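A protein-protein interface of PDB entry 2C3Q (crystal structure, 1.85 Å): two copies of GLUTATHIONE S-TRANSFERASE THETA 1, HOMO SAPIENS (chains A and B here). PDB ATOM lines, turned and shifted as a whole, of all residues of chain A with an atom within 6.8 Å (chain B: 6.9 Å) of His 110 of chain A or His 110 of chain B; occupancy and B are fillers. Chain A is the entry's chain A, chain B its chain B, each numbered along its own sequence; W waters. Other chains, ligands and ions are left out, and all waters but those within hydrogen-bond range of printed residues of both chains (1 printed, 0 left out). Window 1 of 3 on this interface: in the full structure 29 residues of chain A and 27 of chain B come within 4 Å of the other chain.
The guanidinium group of Arg 247 of chain A sits at hydrogen-bond distance from the backbone carbonyl oxygen of Thr 111 of chain B.
O of Trp 108 of chain A lies within hydrogen-bond range of OG1 of Thr 112 of chain A. The backbone carbonyl oxygen (O) of Gln 109 of chain A lies within hydrogen-bond range of the backbone NH (N) of Arg 114 of chain A (3.0 Å). O of Leu 106 of chain B lies within hydrogen-bond range of ND1 of His 110 of chain B, 3.0 Å away. The backbone carbonyl oxygen of Ala 107 of chain B is in hydrogen-bond range of a ring nitrogen (ND1) of His 110 of chain B. NE2 of His 110 of chain B lies close to OE1 of Gln 109 of chain B (3.4 Å). The backbone NH of Arg 114 of chain B sits at hydrogen-bond distance from the backbone carbonyl oxygen of Gln 109 of chain B (2.9 Å).
Ala 107 of chain B touches Glu 73 of chain A. OE2 of Glu 73 of chain A touches CA of Trp 108 of chain B, 3.5 Å away. CB of Ala 107 of chain A touches OE1 of Glu 73 of chain B, 3.6 Å away. CA of Trp 108 of chain A touches OE2 of Glu 73 of chain B, 3.5 Å away. Ala 107 of chain B touches His 110 of chain A (O to CE1, 3.95 Å). His 110 of chain B touches His 110 of chain A (ND1 to CD2, 3.2 Å). Thr 111 of chain B touches His 110 of chain A. Thr 111 of chain A touches His 110 of chain B. Thr 111 of chain A touches Arg 114 of chain B. Arg 114 of chain A touches Thr 111 of chain B.
Printed residues of chain B within 4 Å of Ala 107 of chain A: Glu 73 and His 110. Of chain B, only Ala 107, His 110 and Thr 111 come within 4 Å of His 110 of chain A. Of the printed residues of chain B, Arg 114 of chain A touches Thr 111 (3.5 Å). Ser 116 of chain A touches none of the printed residues of chain B. Printed residues of chain B within 4 Å of Arg 247 of chain A: Thr 111 (2.7 Å) and Arg 115 (3.6 Å). Of the printed residues of chain A, His 110 of chain B touches Ala 107 (3.9 Å), His 110 (3.2 Å) and Thr 111 (3.3 Å). Printed residues of chain A within 4 Å of Arg 114 of chain B: Thr 111. Printed residues of chain A within 4 Å of Arg 115 of chain B: Arg 247. The nearest printed residue of chain B that does not touch Glu 73 of chain A is Tyr 105 of chain B (5.6 Å).
Of the 17 printed residues of chain A, 7 touch a printed residue of chain B. Among the printed residues, 13 pairs touch across the chains. Among the printed residues, no Asp or Glu carboxylate lies within 4 Å of a Lys or Arg side-chain nitrogen of the other chain.
Glu 73 of chain A touches Trp 108 of chain B, and with the chains exchanged Trp 108 of chain A touches Glu 73 of chain B. His 110 of chain B touches its own counterpart, His 110 of chain A. His 110 of chain A touches Thr 111 of chain B, and with the chains exchanged Thr 111 of chain A touches His 110 of chain B. Thr 111 of chain A touches Arg 114 of chain B, and with the chains exchanged Arg 114 of chain A touches Thr 111 of chain B.
Water W1 lies within hydrogen-bond range of O of Thr 112 of chain B, NH2 of Arg 247 of chain A and NH1 of Arg 115 of chain B.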
ATOM      1  N   GLU A  73      -2.519   3.246  23.183  1.00  0.00           N
ATOM      2  CA  GLU A  73      -2.893   1.807  23.266  1.00  0.00           C
ATOM      3  C   GLU A  73      -4.060   1.614  24.209  1.00  0.00           C
ATOM      4  O   GLU A  73      -3.945   1.863  25.400  1.00  0.00           O
ATOM      5  CB  GLU A  73      -1.703   0.906  23.671  1.00  0.00           C
ATOM      6  CG  GLU A  73      -0.565   0.893  22.629  1.00  0.00           C
ATOM      7  CD  GLU A  73      -0.986   0.223  21.331  1.00  0.00           C
ATOM      8  OE1 GLU A  73      -1.780  -0.755  21.352  1.00  0.00           O
ATOM      9  OE2 GLU A  73      -0.494   0.632  20.281  1.00  0.00           O
ATOM     10  N   SER A  74      -5.205   1.198  23.661  1.00  0.00           N
ATOM     11  CA  SER A  74      -6.401   0.961  24.497  1.00  0.00           C
ATOM     12  C   SER A  74      -6.143   0.040  25.687  1.00  0.00           C
ATOM     13  O   SER A  74      -6.645   0.336  26.740  1.00  0.00           O
ATOM     14  CB  SER A  74      -7.552   0.374  23.674  1.00  0.00           C
ATOM     15  OG  SER A  74      -7.130  -0.805  23.010  1.00  0.00           O
ATOM     16  N   VAL A  75      -5.327  -1.024  25.548  1.00  0.00           N
ATOM     17  CA  VAL A  75      -5.092  -1.939  26.698  1.00  0.00           C
ATOM     18  C   VAL A  75      -4.374  -1.163  27.824  1.00  0.00           C
ATOM     19  O   VAL A  75      -4.768  -1.269  28.984  1.00  0.00           O
ATOM     20  CB  VAL A  75      -4.378  -3.275  26.272  1.00  0.00           C
ATOM     21  CG1 VAL A  75      -3.894  -4.111  27.480  1.00  0.00           C
ATOM     22  CG2 VAL A  75      -5.313  -4.077  25.399  1.00  0.00           C
ATOM     23  N   TYR A 105      -6.264 -13.159  27.370  1.00  0.00           N
ATOM     24  CA  TYR A 105      -7.179 -12.678  26.326  1.00  0.00           C
ATOM     25  C   TYR A 105      -6.669 -11.361  25.679  1.00  0.00           C
ATOM     26  O   TYR A 105      -6.630 -11.277  24.454  1.00  0.00           O
ATOM     27  CB  TYR A 105      -8.661 -12.501  26.804  1.00  0.00           C
ATOM     28  CG  TYR A 105      -9.464 -12.006  25.637  1.00  0.00           C
ATOM     29  CD1 TYR A 105      -9.836 -12.893  24.627  1.00  0.00           C
ATOM     30  CD2 TYR A 105      -9.744 -10.619  25.464  1.00  0.00           C
ATOM     31  CE1 TYR A 105     -10.486 -12.437  23.505  1.00  0.00           C
ATOM     32  CE2 TYR A 105     -10.388 -10.162  24.340  1.00  0.00           C
ATOM     33  CZ  TYR A 105     -10.767 -11.087  23.382  1.00  0.00           C
ATOM     34  OH  TYR A 105     -11.371 -10.680  22.254  1.00  0.00           O
ATOM     35  N   LEU A 106      -6.307 -10.378  26.501  1.00  0.00           N
ATOM     36  CA  LEU A 106      -5.872  -9.050  26.024  1.00  0.00           C
ATOM     37  C   LEU A 106      -4.674  -9.174  25.105  1.00  0.00           C
ATOM     38  O   LEU A 106      -4.599  -8.457  24.121  1.00  0.00           O
ATOM     39  CB  LEU A 106      -5.555  -8.088  27.180  1.00  0.00           C
ATOM     40  CG  LEU A 106      -6.730  -7.673  28.106  1.00  0.00           C
ATOM     41  CD1 LEU A 106      -6.178  -6.785  29.203  1.00  0.00           C
ATOM     42  CD2 LEU A 106      -7.859  -6.997  27.367  1.00  0.00           C
ATOM     43  N   ALA A 107      -3.792 -10.126  25.387  1.00  0.00           N
ATOM     44  CA  ALA A 107      -2.624 -10.338  24.541  1.00  0.00           C
ATOM     45  C   ALA A 107      -3.010 -11.023  23.221  1.00  0.00           C
ATOM     46  O   ALA A 107      -2.637 -10.575  22.138  1.00  0.00           O
ATOM     47  CB  ALA A 107      -1.545 -11.130  25.305  1.00  0.00           C
ATOM     48  N   TRP A 108      -3.771 -12.108  23.316  1.00  0.00           N
ATOM     49  CA  TRP A 108      -4.194 -12.869  22.148  1.00  0.00           C
ATOM     50  C   TRP A 108      -4.939 -12.068  21.069  1.00  0.00           C
ATOM     51  O   TRP A 108      -4.624 -12.189  19.881  1.00  0.00           O
ATOM     52  CB  TRP A 108      -5.085 -14.029  22.648  1.00  0.00           C
ATOM     53  CG  TRP A 108      -5.677 -14.890  21.564  1.00  0.00           C
ATOM     54  CD1 TRP A 108      -5.081 -15.954  20.931  1.00  0.00           C
ATOM     55  CD2 TRP A 108      -6.988 -14.761  20.994  1.00  0.00           C
ATOM     56  NE1 TRP A 108      -5.946 -16.484  20.004  1.00  0.00           N
ATOM     57  CE2 TRP A 108      -7.122 -15.776  20.024  1.00  0.00           C
ATOM     58  CE3 TRP A 108      -8.070 -13.890  21.227  1.00  0.00           C
ATOM     59  CZ2 TRP A 108      -8.291 -15.943  19.264  1.00  0.00           C
ATOM     60  CZ3 TRP A 108      -9.237 -14.051  20.480  1.00  0.00           C
ATOM     61  CH2 TRP A 108      -9.328 -15.065  19.494  1.00  0.00           C
ATOM     62  N   GLN A 109      -5.896 -11.243  21.491  1.00  0.00           N
ATOM     63  CA  GLN A 109      -6.815 -10.546  20.574  1.00  0.00           C
ATOM     64  C   GLN A 109      -6.140  -9.584  19.594  1.00  0.00           C
ATOM     65  O   GLN A 109      -6.638  -9.451  18.502  1.00  0.00           O
ATOM     66  CB  GLN A 109      -7.918  -9.793  21.368  1.00  0.00           C
ATOM     67  CG  GLN A 109      -7.526  -8.764  22.424  1.00  0.00           C
ATOM     68  CD  GLN A 109      -7.080  -7.381  21.906  1.00  0.00           C
ATOM     69  OE1 GLN A 109      -6.217  -6.763  22.501  1.00  0.00           O
ATOM     70  NE2 GLN A 109      -7.651  -6.913  20.806  1.00  0.00           N
ATOM     71  N   HIS A 110      -4.990  -9.001  19.975  1.00  0.00           N
ATOM     72  CA  HIS A 110      -4.305  -8.009  19.120  1.00  0.00           C
ATOM     73  C   HIS A 110      -4.070  -8.494  17.682  1.00  0.00           C
ATOM     74  O   HIS A 110      -4.339  -7.754  16.733  1.00  0.00           O
ATOM     75  CB  HIS A 110      -2.962  -7.602  19.696  1.00  0.00           C
ATOM     76  CG  HIS A 110      -3.031  -6.770  20.939  1.00  0.00           C
ATOM     77  ND1 HIS A 110      -3.468  -5.462  20.948  1.00  0.00           N
ATOM     78  CD2 HIS A 110      -2.644  -7.043  22.202  1.00  0.00           C
ATOM     79  CE1 HIS A 110      -3.390  -4.986  22.177  1.00  0.00           C
ATOM     80  NE2 HIS A 110      -2.875  -5.924  22.955  1.00  0.00           N
ATOM     81  N   THR A 111      -3.667  -9.761  17.530  1.00  0.00           N
ATOM     82  CA  THR A 111      -3.294 -10.326  16.232  1.00  0.00           C
ATOM     83  C   THR A 111      -4.310 -11.285  15.624  1.00  0.00           C
ATOM     84  O   THR A 111      -4.059 -11.831  14.561  1.00  0.00           O
ATOM     85  CB  THR A 111      -1.923 -11.079  16.347  1.00  0.00           C
ATOM     86  OG1 THR A 111      -2.019 -12.124  17.313  1.00  0.00           O
ATOM     87  CG2 THR A 111      -0.795 -10.115  16.745  1.00  0.00           C
ATOM     88  N   THR A 112      -5.471 -11.446  16.275  1.00  0.00           N
ATOM     89  CA  THR A 112      -6.442 -12.461  15.888  1.00  0.00           C
ATOM     90  C   THR A 112      -7.817 -11.807  15.732  1.00  0.00           C
ATOM     91  O   THR A 112      -8.138 -11.371  14.637  1.00  0.00           O
ATOM     92  CB  THR A 112      -6.443 -13.627  16.910  1.00  0.00           C
ATOM     93  OG1 THR A 112      -6.737 -13.117  18.205  1.00  0.00           O
ATOM     94  CG2 THR A 112      -5.072 -14.411  16.991  1.00  0.00           C
ATOM     95  N   LEU A 113      -8.578 -11.649  16.814  1.00  0.00           N
ATOM     96  CA  LEU A 113      -9.936 -11.064  16.728  1.00  0.00           C
ATOM     97  C   LEU A 113      -9.942  -9.583  16.316  1.00  0.00           C
ATOM     98  O   LEU A 113     -10.732  -9.206  15.461  1.00  0.00           O
ATOM     99  CB  LEU A 113     -10.696 -11.244  18.052  1.00  0.00           C
ATOM    100  CG  LEU A 113     -12.212 -11.025  17.951  1.00  0.00           C
ATOM    101  CD1 LEU A 113     -12.903 -11.984  16.933  1.00  0.00           C
ATOM    102  CD2 LEU A 113     -12.856 -11.152  19.316  1.00  0.00           C
ATOM    103  N   ARG A 114      -9.070  -8.757  16.903  1.00  0.00           N
ATOM    104  CA  ARG A 114      -8.954  -7.352  16.499  1.00  0.00           C
ATOM    105  C   ARG A 114      -8.763  -7.210  14.976  1.00  0.00           C
ATOM    106  O   ARG A 114      -9.483  -6.439  14.309  1.00  0.00           O
ATOM    107  CB  ARG A 114      -7.798  -6.626  17.212  1.00  0.00           C
ATOM    108  CG  ARG A 114      -7.662  -5.178  16.750  1.00  0.00           C
ATOM    109  CD  ARG A 114      -6.237  -4.612  16.801  1.00  0.00           C
ATOM    110  NE  ARG A 114      -5.333  -5.345  15.923  1.00  0.00           N
ATOM    111  CZ  ARG A 114      -5.025  -5.061  14.662  1.00  0.00           C
ATOM    112  NH1 ARG A 114      -5.523  -4.004  14.048  1.00  0.00           N
ATOM    113  NH2 ARG A 114      -4.190  -5.868  14.008  1.00  0.00           N
ATOM    114  N   ARG A 115      -7.834  -8.004  14.447  1.00  0.00           N
ATOM    115  CA  ARG A 115      -7.449  -7.994  13.042  1.00  0.00           C
ATOM    116  C   ARG A 115      -8.591  -8.439  12.131  1.00  0.00           C
ATOM    117  O   ARG A 115      -8.839  -7.776  11.118  1.00  0.00           O
ATOM    118  CB  ARG A 115      -6.212  -8.885  12.854  1.00  0.00           C
ATOM    119  CG  ARG A 115      -5.724  -8.940  11.435  1.00  0.00           C
ATOM    120  CD  ARG A 115      -4.578  -9.937  11.238  1.00  0.00           C
ATOM    121  NE  ARG A 115      -4.251 -10.019   9.821  1.00  0.00           N
ATOM    122  CZ  ARG A 115      -4.876 -10.809   8.941  1.00  0.00           C
ATOM    123  NH1 ARG A 115      -5.872 -11.619   9.319  1.00  0.00           N
ATOM    124  NH2 ARG A 115      -4.501 -10.797   7.670  1.00  0.00           N
ATOM    125  N   SER A 116      -9.279  -9.531  12.495  1.00  0.00           N
ATOM    126  CA  SER A 116     -10.411 -10.049  11.688  1.00  0.00           C
ATOM    127  C   SER A 116     -11.608  -9.138  11.682  1.00  0.00           C
ATOM    128  O   SER A 116     -12.230  -8.966  10.642  1.00  0.00           O
ATOM    129  CB  SER A 116     -10.881 -11.393  12.204  1.00  0.00           C
ATOM    130  OG  SER A 116      -9.923 -12.341  11.838  1.00  0.00           O
ATOM    131  N   GLU A 180     -15.043  -5.330  19.782  1.00  0.00           N
ATOM    132  CA  GLU A 180     -14.459  -5.900  18.570  1.00  0.00           C
ATOM    133  C   GLU A 180     -15.523  -6.556  17.708  1.00  0.00           C
ATOM    134  O   GLU A 180     -15.617  -6.224  16.533  1.00  0.00           O
ATOM    135  CB  GLU A 180     -13.353  -6.916  18.892  1.00  0.00           C
ATOM    136  CG  GLU A 180     -12.064  -6.150  19.254  1.00  0.00           C
ATOM    137  CD  GLU A 180     -10.970  -6.982  19.866  1.00  0.00           C
ATOM    138  OE1 GLU A 180     -11.214  -8.074  20.424  1.00  0.00           O
ATOM    139  OE2 GLU A 180      -9.833  -6.481  19.835  1.00  0.00           O
ATOM    140  N   ARG A 247      -3.299  -4.682   6.013  1.00  0.00           N
ATOM    141  CA  ARG A 247      -2.105  -5.202   5.328  1.00  0.00           C
ATOM    142  C   ARG A 247      -2.343  -6.397   4.393  1.00  0.00           C
ATOM    143  O   ARG A 247      -3.410  -7.009   4.365  1.00  0.00           O
ATOM    144  CB  ARG A 247      -1.091  -5.576   6.401  1.00  0.00           C
ATOM    145  CG  ARG A 247      -0.529  -4.381   7.114  1.00  0.00           C
ATOM    146  CD  ARG A 247      -0.360  -4.788   8.527  1.00  0.00           C
ATOM    147  NE  ARG A 247       0.549  -3.939   9.268  1.00  0.00           N
ATOM    148  CZ  ARG A 247       0.722  -4.036  10.580  1.00  0.00           C
ATOM    149  NH1 ARG A 247       0.020  -4.926  11.289  1.00  0.00           N
ATOM    150  NH2 ARG A 247       1.585  -3.229  11.193  1.00  0.00           N
ATOM    151  OXT ARG A 247      -1.456  -6.768   3.612  1.00  0.00           O
ATOM    152  N   GLU B  73       0.309 -17.194  25.889  1.00  0.00           N
ATOM    153  CA  GLU B  73       0.689 -15.783  25.579  1.00  0.00           C
ATOM    154  C   GLU B  73       1.875 -15.344  26.382  1.00  0.00           C
ATOM    155  O   GLU B  73       1.812 -15.287  27.602  1.00  0.00           O
ATOM    156  CB  GLU B  73      -0.457 -14.772  25.790  1.00  0.00           C
ATOM    157  CG  GLU B  73      -1.623 -14.955  24.809  1.00  0.00           C
ATOM    158  CD  GLU B  73      -1.240 -14.667  23.350  1.00  0.00           C
ATOM    159  OE1 GLU B  73      -0.431 -13.752  23.065  1.00  0.00           O
ATOM    160  OE2 GLU B  73      -1.781 -15.351  22.493  1.00  0.00           O
ATOM    161  N   SER B  74       2.946 -14.970  25.691  1.00  0.00           N
ATOM    162  CA  SER B  74       4.197 -14.607  26.384  1.00  0.00           C
ATOM    163  C   SER B  74       4.067 -13.403  27.299  1.00  0.00           C
ATOM    164  O   SER B  74       4.676 -13.406  28.351  1.00  0.00           O
ATOM    165  CB  SER B  74       5.344 -14.342  25.382  1.00  0.00           C
ATOM    166  OG  SER B  74       4.971 -13.346  24.456  1.00  0.00           O
ATOM    167  N   VAL B  75       3.280 -12.403  26.908  1.00  0.00           N
ATOM    168  CA  VAL B  75       3.003 -11.228  27.760  1.00  0.00           C
ATOM    169  C   VAL B  75       2.291 -11.664  29.079  1.00  0.00           C
ATOM    170  O   VAL B  75       2.693 -11.243  30.161  1.00  0.00           O
ATOM    171  CB  VAL B  75       2.235 -10.116  26.980  1.00  0.00           C
ATOM    172  CG1 VAL B  75       1.782  -8.999  27.914  1.00  0.00           C
ATOM    173  CG2 VAL B  75       3.104  -9.572  25.838  1.00  0.00           C
ATOM    174  N   TYR B 105       4.102  -0.246  25.439  1.00  0.00           N
ATOM    175  CA  TYR B 105       5.017  -1.029  24.566  1.00  0.00           C
ATOM    176  C   TYR B 105       4.504  -2.463  24.342  1.00  0.00           C
ATOM    177  O   TYR B 105       4.412  -2.904  23.207  1.00  0.00           O
ATOM    178  CB  TYR B 105       6.492  -1.088  25.061  1.00  0.00           C
ATOM    179  CG  TYR B 105       7.262  -1.828  24.021  1.00  0.00           C
ATOM    180  CD1 TYR B 105       7.579  -1.196  22.821  1.00  0.00           C
ATOM    181  CD2 TYR B 105       7.546  -3.210  24.146  1.00  0.00           C
ATOM    182  CE1 TYR B 105       8.174  -1.884  21.789  1.00  0.00           C
ATOM    183  CE2 TYR B 105       8.164  -3.900  23.115  1.00  0.00           C
ATOM    184  CZ  TYR B 105       8.473  -3.218  21.955  1.00  0.00           C
ATOM    185  OH  TYR B 105       9.053  -3.850  20.922  1.00  0.00           O
ATOM    186  N   LEU B 106       4.215  -3.183  25.420  1.00  0.00           N
ATOM    187  CA  LEU B 106       3.711  -4.585  25.339  1.00  0.00           C
ATOM    188  C   LEU B 106       2.480  -4.698  24.436  1.00  0.00           C
ATOM    189  O   LEU B 106       2.381  -5.630  23.645  1.00  0.00           O
ATOM    190  CB  LEU B 106       3.420  -5.136  26.734  1.00  0.00           C
ATOM    191  CG  LEU B 106       4.673  -5.352  27.614  1.00  0.00           C
ATOM    192  CD1 LEU B 106       4.214  -5.846  28.980  1.00  0.00           C
ATOM    193  CD2 LEU B 106       5.689  -6.296  26.993  1.00  0.00           C
ATOM    194  N   ALA B 107       1.582  -3.715  24.506  1.00  0.00           N
ATOM    195  CA  ALA B 107       0.406  -3.706  23.612  1.00  0.00           C
ATOM    196  C   ALA B 107       0.755  -3.365  22.162  1.00  0.00           C
ATOM    197  O   ALA B 107       0.351  -4.090  21.264  1.00  0.00           O
ATOM    198  CB  ALA B 107      -0.682  -2.748  24.156  1.00  0.00           C
ATOM    199  N   TRP B 108       1.562  -2.319  21.953  1.00  0.00           N
ATOM    200  CA  TRP B 108       1.942  -1.849  20.618  1.00  0.00           C
ATOM    201  C   TRP B 108       2.664  -2.881  19.751  1.00  0.00           C
ATOM    202  O   TRP B 108       2.329  -3.028  18.576  1.00  0.00           O
ATOM    203  CB  TRP B 108       2.819  -0.577  20.753  1.00  0.00           C
ATOM    204  CG  TRP B 108       3.373  -0.032  19.455  1.00  0.00           C
ATOM    205  CD1 TRP B 108       2.751   0.857  18.596  1.00  0.00           C
ATOM    206  CD2 TRP B 108       4.653  -0.327  18.865  1.00  0.00           C
ATOM    207  NE1 TRP B 108       3.567   1.122  17.525  1.00  0.00           N
ATOM    208  CE2 TRP B 108       4.740   0.419  17.669  1.00  0.00           C
ATOM    209  CE3 TRP B 108       5.751  -1.132  19.249  1.00  0.00           C
ATOM    210  CZ2 TRP B 108       5.872   0.378  16.844  1.00  0.00           C
ATOM    211  CZ3 TRP B 108       6.886  -1.175  18.417  1.00  0.00           C
ATOM    212  CH2 TRP B 108       6.928  -0.425  17.235  1.00  0.00           C
ATOM    213  N   GLN B 109       3.614  -3.613  20.346  1.00  0.00           N
ATOM    214  CA  GLN B 109       4.529  -4.536  19.610  1.00  0.00           C
ATOM    215  C   GLN B 109       3.860  -5.713  18.914  1.00  0.00           C
ATOM    216  O   GLN B 109       4.372  -6.149  17.907  1.00  0.00           O
ATOM    217  CB  GLN B 109       5.668  -5.057  20.553  1.00  0.00           C
ATOM    218  CG  GLN B 109       5.246  -5.772  21.841  1.00  0.00           C
ATOM    219  CD  GLN B 109       4.787  -7.233  21.689  1.00  0.00           C
ATOM    220  OE1 GLN B 109       3.945  -7.695  22.448  1.00  0.00           O
ATOM    221  NE2 GLN B 109       5.343  -7.951  20.729  1.00  0.00           N
ATOM    222  N   HIS B 110       2.728  -6.197  19.451  1.00  0.00           N
ATOM    223  CA  HIS B 110       2.013  -7.373  18.877  1.00  0.00           C
ATOM    224  C   HIS B 110       1.741  -7.291  17.381  1.00  0.00           C
ATOM    225  O   HIS B 110       1.963  -8.253  16.665  1.00  0.00           O
ATOM    226  CB  HIS B 110       0.670  -7.574  19.563  1.00  0.00           C
ATOM    227  CG  HIS B 110       0.764  -8.119  20.945  1.00  0.00           C
ATOM    228  ND1 HIS B 110       0.527  -7.355  22.070  1.00  0.00           N
ATOM    229  CD2 HIS B 110       1.044  -9.366  21.383  1.00  0.00           C
ATOM    230  CE1 HIS B 110       0.628  -8.129  23.140  1.00  0.00           C
ATOM    231  NE2 HIS B 110       0.966  -9.344  22.751  1.00  0.00           N
ATOM    232  N   THR B 111       1.322  -6.110  16.929  1.00  0.00           N
ATOM    233  CA  THR B 111       0.868  -5.892  15.559  1.00  0.00           C
ATOM    234  C   THR B 111       1.865  -5.116  14.696  1.00  0.00           C
ATOM    235  O   THR B 111       1.589  -4.826  13.518  1.00  0.00           O
ATOM    236  CB  THR B 111      -0.491  -5.147  15.585  1.00  0.00           C
ATOM    237  OG1 THR B 111      -0.354  -3.927  16.294  1.00  0.00           O
ATOM    238  CG2 THR B 111      -1.547  -5.984  16.283  1.00  0.00           C
ATOM    239  N   THR B 112       3.026  -4.808  15.269  1.00  0.00           N
ATOM    240  CA  THR B 112       4.020  -3.973  14.601  1.00  0.00           C
ATOM    241  C   THR B 112       5.397  -4.645  14.543  1.00  0.00           C
ATOM    242  O   THR B 112       5.709  -5.299  13.554  1.00  0.00           O
ATOM    243  CB  THR B 112       4.112  -2.578  15.290  1.00  0.00           C
ATOM    244  OG1 THR B 112       4.409  -2.741  16.677  1.00  0.00           O
ATOM    245  CG2 THR B 112       2.792  -1.756  15.138  1.00  0.00           C
ATOM    246  N   LEU B 113       6.188  -4.515  15.606  1.00  0.00           N
ATOM    247  CA  LEU B 113       7.555  -5.059  15.635  1.00  0.00           C
ATOM    248  C   LEU B 113       7.536  -6.598  15.672  1.00  0.00           C
ATOM    249  O   LEU B 113       8.335  -7.225  14.977  1.00  0.00           O
ATOM    250  CB  LEU B 113       8.363  -4.452  16.802  1.00  0.00           C
ATOM    251  CG  LEU B 113       9.876  -4.720  16.763  1.00  0.00           C
ATOM    252  CD1 LEU B 113      10.585  -3.960  15.617  1.00  0.00           C
ATOM    253  CD2 LEU B 113      10.514  -4.367  18.089  1.00  0.00           C
ATOM    254  N   ARG B 114       6.602  -7.203  16.417  1.00  0.00           N
ATOM    255  CA  ARG B 114       6.496  -8.672  16.400  1.00  0.00           C
ATOM    256  C   ARG B 114       6.344  -9.181  14.967  1.00  0.00           C
ATOM    257  O   ARG B 114       7.089 -10.060  14.533  1.00  0.00           O
ATOM    258  CB  ARG B 114       5.324  -9.193  17.243  1.00  0.00           C
ATOM    259  CG  ARG B 114       5.180 -10.716  17.199  1.00  0.00           C
ATOM    260  CD  ARG B 114       3.748 -11.198  17.424  1.00  0.00           C
ATOM    261  NE  ARG B 114       2.829 -10.721  16.390  1.00  0.00           N
ATOM    262  CZ  ARG B 114       2.571 -11.329  15.230  1.00  0.00           C
ATOM    263  NH1 ARG B 114       3.159 -12.471  14.907  1.00  0.00           N
ATOM    264  NH2 ARG B 114       1.717 -10.783  14.372  1.00  0.00           N
ATOM    265  N   ARG B 115       5.391  -8.596  14.251  1.00  0.00           N
ATOM    266  CA  ARG B 115       5.046  -8.995  12.885  1.00  0.00           C
ATOM    267  C   ARG B 115       6.202  -8.769  11.895  1.00  0.00           C
ATOM    268  O   ARG B 115       6.577  -9.657  11.141  1.00  0.00           O
ATOM    269  CB  ARG B 115       3.792  -8.234  12.457  1.00  0.00           C
ATOM    270  CG  ARG B 115       3.331  -8.553  11.053  1.00  0.00           C
ATOM    271  CD  ARG B 115       2.129  -7.736  10.664  1.00  0.00           C
ATOM    272  NE  ARG B 115       1.712  -8.055   9.296  1.00  0.00           N
ATOM    273  CZ  ARG B 115       2.154  -7.435   8.211  1.00  0.00           C
ATOM    274  NH1 ARG B 115       3.058  -6.455   8.312  1.00  0.00           N
ATOM    275  NH2 ARG B 115       1.700  -7.817   7.017  1.00  0.00           N
ATOM    276  N   SER B 116       6.781  -7.575  11.960  1.00  0.00           N
ATOM    277  CA  SER B 116       7.887  -7.196  11.124  1.00  0.00           C
ATOM    278  C   SER B 116       9.157  -8.051  11.276  1.00  0.00           C
ATOM    279  O   SER B 116       9.832  -8.355  10.279  1.00  0.00           O
ATOM    280  CB  SER B 116       8.242  -5.770  11.475  1.00  0.00           C
ATOM    281  OG  SER B 116       9.184  -5.410  10.540  1.00  0.00           O
ATOM    282  N   VAL B 176      11.004  -8.010  25.694  1.00  0.00           N
ATOM    283  CA  VAL B 176      10.219  -8.368  24.516  1.00  0.00           C
ATOM    284  C   VAL B 176      10.834  -7.769  23.237  1.00  0.00           C
ATOM    285  O   VAL B 176      11.027  -8.483  22.259  1.00  0.00           O
ATOM    286  CB  VAL B 176       8.702  -7.967  24.715  1.00  0.00           C
ATOM    287  CG1 VAL B 176       7.912  -8.183  23.473  1.00  0.00           C
ATOM    288  CG2 VAL B 176       8.125  -8.765  25.868  1.00  0.00           C
ATOM    289  N   GLU B 180      12.733  -9.781  19.972  1.00  0.00           N
ATOM    290  CA  GLU B 180      12.125  -9.536  18.653  1.00  0.00           C
ATOM    291  C   GLU B 180      13.196  -9.122  17.666  1.00  0.00           C
ATOM    292  O   GLU B 180      13.327  -9.749  16.615  1.00  0.00           O
ATOM    293  CB  GLU B 180      11.006  -8.486  18.740  1.00  0.00           C
ATOM    294  CG  GLU B 180       9.749  -9.133  19.301  1.00  0.00           C
ATOM    295  CD  GLU B 180       8.628  -8.187  19.684  1.00  0.00           C
ATOM    296  OE1 GLU B 180       8.828  -6.958  19.918  1.00  0.00           O
ATOM    297  OE2 GLU B 180       7.517  -8.743  19.768  1.00  0.00           O
HETATM  298  O   HOH W   1       4.647  -4.808  10.918  1.00  0.00           O
